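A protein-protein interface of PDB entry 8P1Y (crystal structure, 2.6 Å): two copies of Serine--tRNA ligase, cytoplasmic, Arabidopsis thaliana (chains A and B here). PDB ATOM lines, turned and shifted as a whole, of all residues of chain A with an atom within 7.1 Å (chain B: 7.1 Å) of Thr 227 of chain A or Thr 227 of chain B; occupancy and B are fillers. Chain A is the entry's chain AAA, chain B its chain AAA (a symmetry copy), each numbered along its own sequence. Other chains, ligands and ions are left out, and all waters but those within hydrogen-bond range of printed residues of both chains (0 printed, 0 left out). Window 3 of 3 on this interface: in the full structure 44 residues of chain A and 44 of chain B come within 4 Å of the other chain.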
ATOM      1  N   TYR A 224     -22.589  17.063 -10.348  1.00  0.00           N
ATOM      2  CA  TYR A 224     -22.158  17.479  -8.990  1.00  0.00           C
ATOM      3  C   TYR A 224     -20.624  17.584  -8.988  1.00  0.00           C
ATOM      4  O   TYR A 224     -19.966  16.786  -9.708  1.00  0.00           O
ATOM      5  CB  TYR A 224     -22.702  16.504  -7.941  1.00  0.00           C
ATOM      6  CG  TYR A 224     -24.173  16.659  -7.641  1.00  0.00           C
ATOM      7  CD1 TYR A 224     -24.604  17.599  -6.717  1.00  0.00           C
ATOM      8  CD2 TYR A 224     -25.136  15.877  -8.263  1.00  0.00           C
ATOM      9  CE1 TYR A 224     -25.947  17.763  -6.419  1.00  0.00           C
ATOM     10  CE2 TYR A 224     -26.486  16.039  -7.985  1.00  0.00           C
ATOM     11  CZ  TYR A 224     -26.893  16.986  -7.061  1.00  0.00           C
ATOM     12  OH  TYR A 224     -28.208  17.167  -6.744  1.00  0.00           O
ATOM     13  N   LYS A 225     -20.087  18.555  -8.234  1.00  0.00           N
ATOM     14  CA  LYS A 225     -18.626  18.783  -8.043  1.00  0.00           C
ATOM     15  C   LYS A 225     -18.219  18.271  -6.651  1.00  0.00           C
ATOM     16  O   LYS A 225     -18.975  18.504  -5.687  1.00  0.00           O
ATOM     17  CB  LYS A 225     -18.307  20.274  -8.223  1.00  0.00           C
ATOM     18  CG  LYS A 225     -17.023  20.587  -8.990  1.00  0.00           C
ATOM     19  CD  LYS A 225     -16.620  22.071  -9.018  1.00  0.00           C
ATOM     20  CE  LYS A 225     -17.478  22.938  -9.923  1.00  0.00           C
ATOM     21  NZ  LYS A 225     -17.395  22.534 -11.349  1.00  0.00           N
ATOM     22  N   VAL A 226     -17.067  17.609  -6.539  1.00  0.00           N
ATOM     23  CA  VAL A 226     -16.550  17.069  -5.242  1.00  0.00           C
ATOM     24  C   VAL A 226     -15.181  17.689  -4.928  1.00  0.00           C
ATOM     25  O   VAL A 226     -14.213  17.368  -5.633  1.00  0.00           O
ATOM     26  CB  VAL A 226     -16.474  15.532  -5.266  1.00  0.00           C
ATOM     27  CG1 VAL A 226     -16.177  14.973  -3.884  1.00  0.00           C
ATOM     28  CG2 VAL A 226     -17.744  14.917  -5.824  1.00  0.00           C
ATOM     29  N   THR A 227     -15.100  18.477  -3.853  1.00  0.00           N
ATOM     30  CA  THR A 227     -13.983  19.415  -3.540  1.00  0.00           C
ATOM     31  C   THR A 227     -12.776  18.641  -2.976  1.00  0.00           C
ATOM     32  O   THR A 227     -11.696  18.674  -3.633  1.00  0.00           O
ATOM     33  CB  THR A 227     -14.508  20.534  -2.631  1.00  0.00           C
ATOM     34  OG1 THR A 227     -15.570  21.169  -3.341  1.00  0.00           O
ATOM     35  CG2 THR A 227     -13.457  21.555  -2.260  1.00  0.00           C
ATOM     36  N   GLY A 228     -12.925  18.060  -1.774  1.00  0.00           N
ATOM     37  CA  GLY A 228     -12.260  16.808  -1.343  1.00  0.00           C
ATOM     38  C   GLY A 228     -10.766  16.903  -1.041  1.00  0.00           C
ATOM     39  O   GLY A 228     -10.402  17.694  -0.145  1.00  0.00           O
ATOM     40  N   GLU A 229      -9.955  16.071  -1.728  1.00  0.00           N
ATOM     41  CA  GLU A 229      -8.536  15.735  -1.403  1.00  0.00           C
ATOM     42  C   GLU A 229      -7.579  16.247  -2.494  1.00  0.00           C
ATOM     43  O   GLU A 229      -6.924  17.291  -2.259  1.00  0.00           O
ATOM     44  CB  GLU A 229      -8.371  14.223  -1.206  1.00  0.00           C
ATOM     45  CG  GLU A 229      -8.616  13.766   0.228  1.00  0.00           C
ATOM     46  CD  GLU A 229      -7.524  14.092   1.241  1.00  0.00           C
ATOM     47  OE1 GLU A 229      -6.479  13.414   1.230  1.00  0.00           O
ATOM     48  OE2 GLU A 229      -7.726  15.014   2.055  1.00  0.00           O
ATOM     49  N   GLY A 230      -7.460  15.530  -3.619  1.00  0.00           N
ATOM     50  CA  GLY A 230      -6.620  15.934  -4.767  1.00  0.00           C
ATOM     51  C   GLY A 230      -7.350  16.922  -5.667  1.00  0.00           C
ATOM     52  O   GLY A 230      -8.076  17.792  -5.133  1.00  0.00           O
ATOM     53  N   ASP A 231      -7.181  16.795  -6.990  1.00  0.00           N
ATOM     54  CA  ASP A 231      -7.902  17.611  -8.008  1.00  0.00           C
ATOM     55  C   ASP A 231      -9.386  17.657  -7.648  1.00  0.00           C
ATOM     56  O   ASP A 231      -9.844  16.766  -6.905  1.00  0.00           O
ATOM     57  CB  ASP A 231      -7.748  17.056  -9.428  1.00  0.00           C
ATOM     58  CG  ASP A 231      -6.456  17.449 -10.127  1.00  0.00           C
ATOM     59  OD1 ASP A 231      -5.814  18.442  -9.699  1.00  0.00           O
ATOM     60  OD2 ASP A 231      -6.102  16.756 -11.101  1.00  0.00           O
ATOM     61  N   ASP A 232     -10.095  18.672  -8.145  1.00  0.00           N
ATOM     62  CA  ASP A 232     -11.575  18.739  -8.057  1.00  0.00           C
ATOM     63  C   ASP A 232     -12.098  17.608  -8.949  1.00  0.00           C
ATOM     64  O   ASP A 232     -11.468  17.333 -10.018  1.00  0.00           O
ATOM     65  CB  ASP A 232     -12.112  20.142  -8.363  1.00  0.00           C
ATOM     66  CG  ASP A 232     -12.134  21.072  -7.155  1.00  0.00           C
ATOM     67  OD1 ASP A 232     -11.386  20.811  -6.182  1.00  0.00           O
ATOM     68  OD2 ASP A 232     -12.908  22.050  -7.185  1.00  0.00           O
ATOM     69  N   LYS A 233     -13.143  16.929  -8.460  1.00  0.00           N
ATOM     70  CA  LYS A 233     -13.752  15.711  -9.053  1.00  0.00           C
ATOM     71  C   LYS A 233     -15.243  15.966  -9.292  1.00  0.00           C
ATOM     72  O   LYS A 233     -15.822  16.855  -8.631  1.00  0.00           O
ATOM     73  CB  LYS A 233     -13.601  14.507  -8.115  1.00  0.00           C
ATOM     74  CG  LYS A 233     -12.214  14.274  -7.520  1.00  0.00           C
ATOM     75  CD  LYS A 233     -12.242  13.800  -6.071  1.00  0.00           C
ATOM     76  CE  LYS A 233     -10.899  13.884  -5.378  1.00  0.00           C
ATOM     77  NZ  LYS A 233      -9.831  13.240  -6.180  1.00  0.00           N
ATOM     78  N   LYS A 270     -27.877  16.422 -11.390  1.00  0.00           N
ATOM     79  CA  LYS A 270     -28.335  17.749 -10.888  1.00  0.00           C
ATOM     80  C   LYS A 270     -29.777  17.983 -11.366  1.00  0.00           C
ATOM     81  O   LYS A 270     -30.636  18.319 -10.505  1.00  0.00           O
ATOM     82  CB  LYS A 270     -27.401  18.878 -11.353  1.00  0.00           C
ATOM     83  CG  LYS A 270     -26.080  19.022 -10.603  1.00  0.00           C
ATOM     84  CD  LYS A 270     -25.422  20.386 -10.755  1.00  0.00           C
ATOM     85  CE  LYS A 270     -24.840  20.610 -12.136  1.00  0.00           C
ATOM     86  NZ  LYS A 270     -24.626  22.047 -12.433  1.00  0.00           N
ATOM     87  N   TYR B 224     -15.959  14.987   2.493  1.00  0.00           N
ATOM     88  CA  TYR B 224     -16.057  15.543   1.120  1.00  0.00           C
ATOM     89  C   TYR B 224     -17.204  16.566   1.100  1.00  0.00           C
ATOM     90  O   TYR B 224     -18.206  16.359   1.836  1.00  0.00           O
ATOM     91  CB  TYR B 224     -16.235  14.411   0.103  1.00  0.00           C
ATOM     92  CG  TYR B 224     -14.980  13.624  -0.187  1.00  0.00           C
ATOM     93  CD1 TYR B 224     -14.072  14.076  -1.133  1.00  0.00           C
ATOM     94  CD2 TYR B 224     -14.693  12.433   0.465  1.00  0.00           C
ATOM     95  CE1 TYR B 224     -12.913  13.375  -1.422  1.00  0.00           C
ATOM     96  CE2 TYR B 224     -13.530  11.726   0.195  1.00  0.00           C
ATOM     97  CZ  TYR B 224     -12.637  12.198  -0.751  1.00  0.00           C
ATOM     98  OH  TYR B 224     -11.490  11.527  -1.061  1.00  0.00           O
ATOM     99  N   LYS B 225     -17.041  17.642   0.315  1.00  0.00           N
ATOM    100  CA  LYS B 225     -18.057  18.712   0.105  1.00  0.00           C
ATOM    101  C   LYS B 225     -18.705  18.520  -1.276  1.00  0.00           C
ATOM    102  O   LYS B 225     -17.975  18.214  -2.239  1.00  0.00           O
ATOM    103  CB  LYS B 225     -17.393  20.089   0.242  1.00  0.00           C
ATOM    104  CG  LYS B 225     -18.209  21.145   0.988  1.00  0.00           C
ATOM    105  CD  LYS B 225     -17.617  22.564   0.971  1.00  0.00           C
ATOM    106  CE  LYS B 225     -16.400  22.747   1.860  1.00  0.00           C
ATOM    107  NZ  LYS B 225     -16.699  22.519   3.296  1.00  0.00           N
ATOM    108  N   VAL B 226     -20.022  18.700  -1.381  1.00  0.00           N
ATOM    109  CA  VAL B 226     -20.773  18.555  -2.668  1.00  0.00           C
ATOM    110  C   VAL B 226     -21.478  19.875  -3.012  1.00  0.00           C
ATOM    111  O   VAL B 226     -22.433  20.234  -2.307  1.00  0.00           O
ATOM    112  CB  VAL B 226     -21.775  17.388  -2.602  1.00  0.00           C
ATOM    113  CG1 VAL B 226     -22.365  17.092  -3.972  1.00  0.00           C
ATOM    114  CG2 VAL B 226     -21.144  16.139  -2.017  1.00  0.00           C
ATOM    115  N   THR B 227     -21.069  20.518  -4.109  1.00  0.00           N
ATOM    116  CA  THR B 227     -21.379  21.935  -4.457  1.00  0.00           C
ATOM    117  C   THR B 227     -22.813  22.048  -5.011  1.00  0.00           C
ATOM    118  O   THR B 227     -23.640  22.754  -4.365  1.00  0.00           O
ATOM    119  CB  THR B 227     -20.288  22.472  -5.391  1.00  0.00           C
ATOM    120  OG1 THR B 227     -19.053  22.342  -4.688  1.00  0.00           O
ATOM    121  CG2 THR B 227     -20.495  23.912  -5.799  1.00  0.00           C
ATOM    122  N   GLY B 228     -23.063  21.465  -6.195  1.00  0.00           N
ATOM    123  CA  GLY B 228     -24.359  20.872  -6.598  1.00  0.00           C
ATOM    124  C   GLY B 228     -25.484  21.855  -6.916  1.00  0.00           C
ATOM    125  O   GLY B 228     -25.295  22.678  -7.837  1.00  0.00           O
ATOM    126  N   GLU B 229     -26.628  21.714  -6.214  1.00  0.00           N
ATOM    127  CA  GLU B 229     -27.958  22.310  -6.544  1.00  0.00           C
ATOM    128  C   GLU B 229     -28.391  23.331  -5.476  1.00  0.00           C
ATOM    129  O   GLU B 229     -28.270  24.550  -5.745  1.00  0.00           O
ATOM    130  CB  GLU B 229     -29.017  21.211  -6.701  1.00  0.00           C
ATOM    131  CG  GLU B 229     -29.118  20.662  -8.119  1.00  0.00           C
ATOM    132  CD  GLU B 229     -29.790  21.560  -9.152  1.00  0.00           C
ATOM    133  OE1 GLU B 229     -31.031  21.666  -9.132  1.00  0.00           O
ATOM    134  OE2 GLU B 229     -29.072  22.142  -9.988  1.00  0.00           O
ATOM    135  N   GLY B 230     -28.914  22.868  -4.333  1.00  0.00           N
ATOM    136  CA  GLY B 230     -29.319  23.733  -3.204  1.00  0.00           C
ATOM    137  C   GLY B 230     -28.128  24.090  -2.325  1.00  0.00           C
ATOM    138  O   GLY B 230     -27.027  24.317  -2.875  1.00  0.00           O
ATOM    139  N   ASP B 231     -28.327  24.130  -1.001  1.00  0.00           N
ATOM    140  CA  ASP B 231     -27.248  24.360   0.002  1.00  0.00           C
ATOM    141  C   ASP B 231     -26.050  23.476  -0.345  1.00  0.00           C
ATOM    142  O   ASP B 231     -26.242  22.471  -1.060  1.00  0.00           O
ATOM    143  CB  ASP B 231     -27.696  24.054   1.435  1.00  0.00           C
ATOM    144  CG  ASP B 231     -28.470  25.175   2.110  1.00  0.00           C
ATOM    145  OD1 ASP B 231     -28.372  26.342   1.650  1.00  0.00           O
ATOM    146  OD2 ASP B 231     -29.165  24.872   3.100  1.00  0.00           O
ATOM    147  N   ASP B 232     -24.863  23.857   0.130  1.00  0.00           N
ATOM    148  CA  ASP B 232     -23.655  23.000   0.054  1.00  0.00           C
ATOM    149  C   ASP B 232     -23.926  21.811   0.982  1.00  0.00           C
ATOM    150  O   ASP B 232     -24.582  22.008   2.052  1.00  0.00           O
ATOM    151  CB  ASP B 232     -22.367  23.787   0.327  1.00  0.00           C
ATOM    152  CG  ASP B 232     -21.791  24.475  -0.906  1.00  0.00           C
ATOM    153  OD1 ASP B 232     -22.551  24.700  -1.878  1.00  0.00           O
ATOM    154  OD2 ASP B 232     -20.579  24.773  -0.895  1.00  0.00           O
ATOM    155  N   LYS B 233     -23.521  20.620   0.521  1.00  0.00           N
ATOM    156  CA  LYS B 233     -23.781  19.301   1.152  1.00  0.00           C
ATOM    157  C   LYS B 233     -22.445  18.595   1.398  1.00  0.00           C
ATOM    158  O   LYS B 233     -21.449  18.924   0.719  1.00  0.00           O
ATOM    159  CB  LYS B 233     -24.648  18.417   0.246  1.00  0.00           C
ATOM    160  CG  LYS B 233     -25.891  19.068  -0.355  1.00  0.00           C
ATOM    161  CD  LYS B 233     -26.173  18.637  -1.790  1.00  0.00           C
ATOM    162  CE  LYS B 233     -27.190  19.508  -2.498  1.00  0.00           C
ATOM    163  NZ  LYS B 233     -28.420  19.676  -1.689  1.00  0.00           N
ATOM    164  N   LYS B 270     -12.164  11.267   3.601  1.00  0.00           N
ATOM    165  CA  LYS B 270     -10.993  12.021   3.067  1.00  0.00           C
ATOM    166  C   LYS B 270      -9.706  11.335   3.552  1.00  0.00           C
ATOM    167  O   LYS B 270      -8.830  11.050   2.690  1.00  0.00           O
ATOM    168  CB  LYS B 270     -11.035  13.498   3.493  1.00  0.00           C
ATOM    169  CG  LYS B 270     -11.998  14.401   2.726  1.00  0.00           C
ATOM    170  CD  LYS B 270     -11.680  15.885   2.835  1.00  0.00           C
ATOM    171  CE  LYS B 270     -11.989  16.457   4.204  1.00  0.00           C
ATOM    172  NZ  LYS B 270     -11.275  17.731   4.460  1.00  0.00           N
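The backbone carbonyl oxygen (O) of Lys 225 of chain A lies within hydrogen-bond range of the backbone NH (N) of Thr 227 of chain B. The backbone NH (N) of Thr 227 of chain A sits at hydrogen-bond distance from the backbone carbonyl oxygen (O) of Lys 225 of chain B (3.3 Å).
The backbone NH (N) of Val 226 of chain A lies within hydrogen-bond range of the backbone carbonyl oxygen (O) of Lys 233 of chain A, at 2.5 Å. N of Val 226 of chain B sits at hydrogen-bond distance from O of Lys 233 of chain B (2.5 Å).
Tyr 224 of chain A touches Val 226 of chain B (CD1 to CG1, 3.6 Å). CD1 of Tyr 224 of chain A touches CA of Gly 228 of chain B, 3.3 Å away. Lys 225 of chain B touches Lys 225 of chain A. Lys 225 of chain A touches Val 226 of chain B. O of Lys 225 of chain B touches CA of Val 226 of chain A, 3.5 Å away. Thr 227 of chain A touches Thr 227 of chain B. O of Gly 228 of chain A touches CD of Lys 270 of chain B, at 3.7 Å. Glu 229 of chain A touches Tyr 224 of chain B (CG to OH, 3.9 Å). CD of Lys 270 of chain A touches O of Gly 228 of chain B (3.7 Å). CD of Glu 229 of chain B touches O of Lys 270 of chain A, 3.6 Å away.
Thr 227 of chain A touches just these residues of chain B: Lys 225 (3.3 Å) and Thr 227 (3.9 Å). Thr 227 of chain B touches just these residues of chain A: Lys 225 and Thr 227. Of the printed residues of chain B, Lys 270 of chain A touches Gly 228 (3.7 Å) and Glu 229 (3.6 Å). Of the printed residues of chain B, Lys 225 of chain A touches Lys 225 (3.6 Å), Val 226 (3.5 Å) and Thr 227 (3.3 Å). Printed residues of chain B within 4 Å of Glu 229 of chain A: Tyr 224 (3.9 Å) and Lys 270 (3.6 Å). Gly 230 of chain A touches none of the printed residues of chain B. Lys 233 of chain B touches none of the printed residues of chain A. The nearest residue of chain B that does not touch Thr 227 of chain A is Tyr 224 of chain B (5.1 Å). The nearest residue of chain A that does not touch Thr 227 of chain B is Tyr 224 of chain A (5.1 Å). The nearest printed residue of chain A that does not touch Gly 228 of chain B is Lys 225 of chain A (4.6 Å).
Of the 11 printed residues of chain B, 7 touch a printed residue of chain A. Printed residues of chain B that touch a printed residue of chain A: Tyr 224, Lys 225, Val 226, Thr 227, Gly 228, Glu 229 and Lys 270. Hydrophobic or aromatic side chains of chain B that line the printed part of chain A: Tyr 224 and Val 226. Along chain B the printed residues that touch a printed residue of chain A span positions 224 to 270. Among the printed residues, 16 pairs touch across the chains.
Tyr 224 of chain A touches Gly 228 of chain B, and with the chains exchanged Gly 228 of chain A touches Tyr 224 of chain B. Tyr 224 of chain A touches Glu 229 of chain B, and with the chains exchanged Glu 229 of chain A touches Tyr 224 of chain B. Lys 225 of chain A touches Thr 227 of chain B, and with the chains exchanged Thr 227 of chain A touches Lys 225 of chain B. Glu 229 of chain A touches Lys 270 of chain B, and with the chains exchanged Lys 270 of chain A touches Glu 229 of chain B. 11 positions are printed for both chains.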
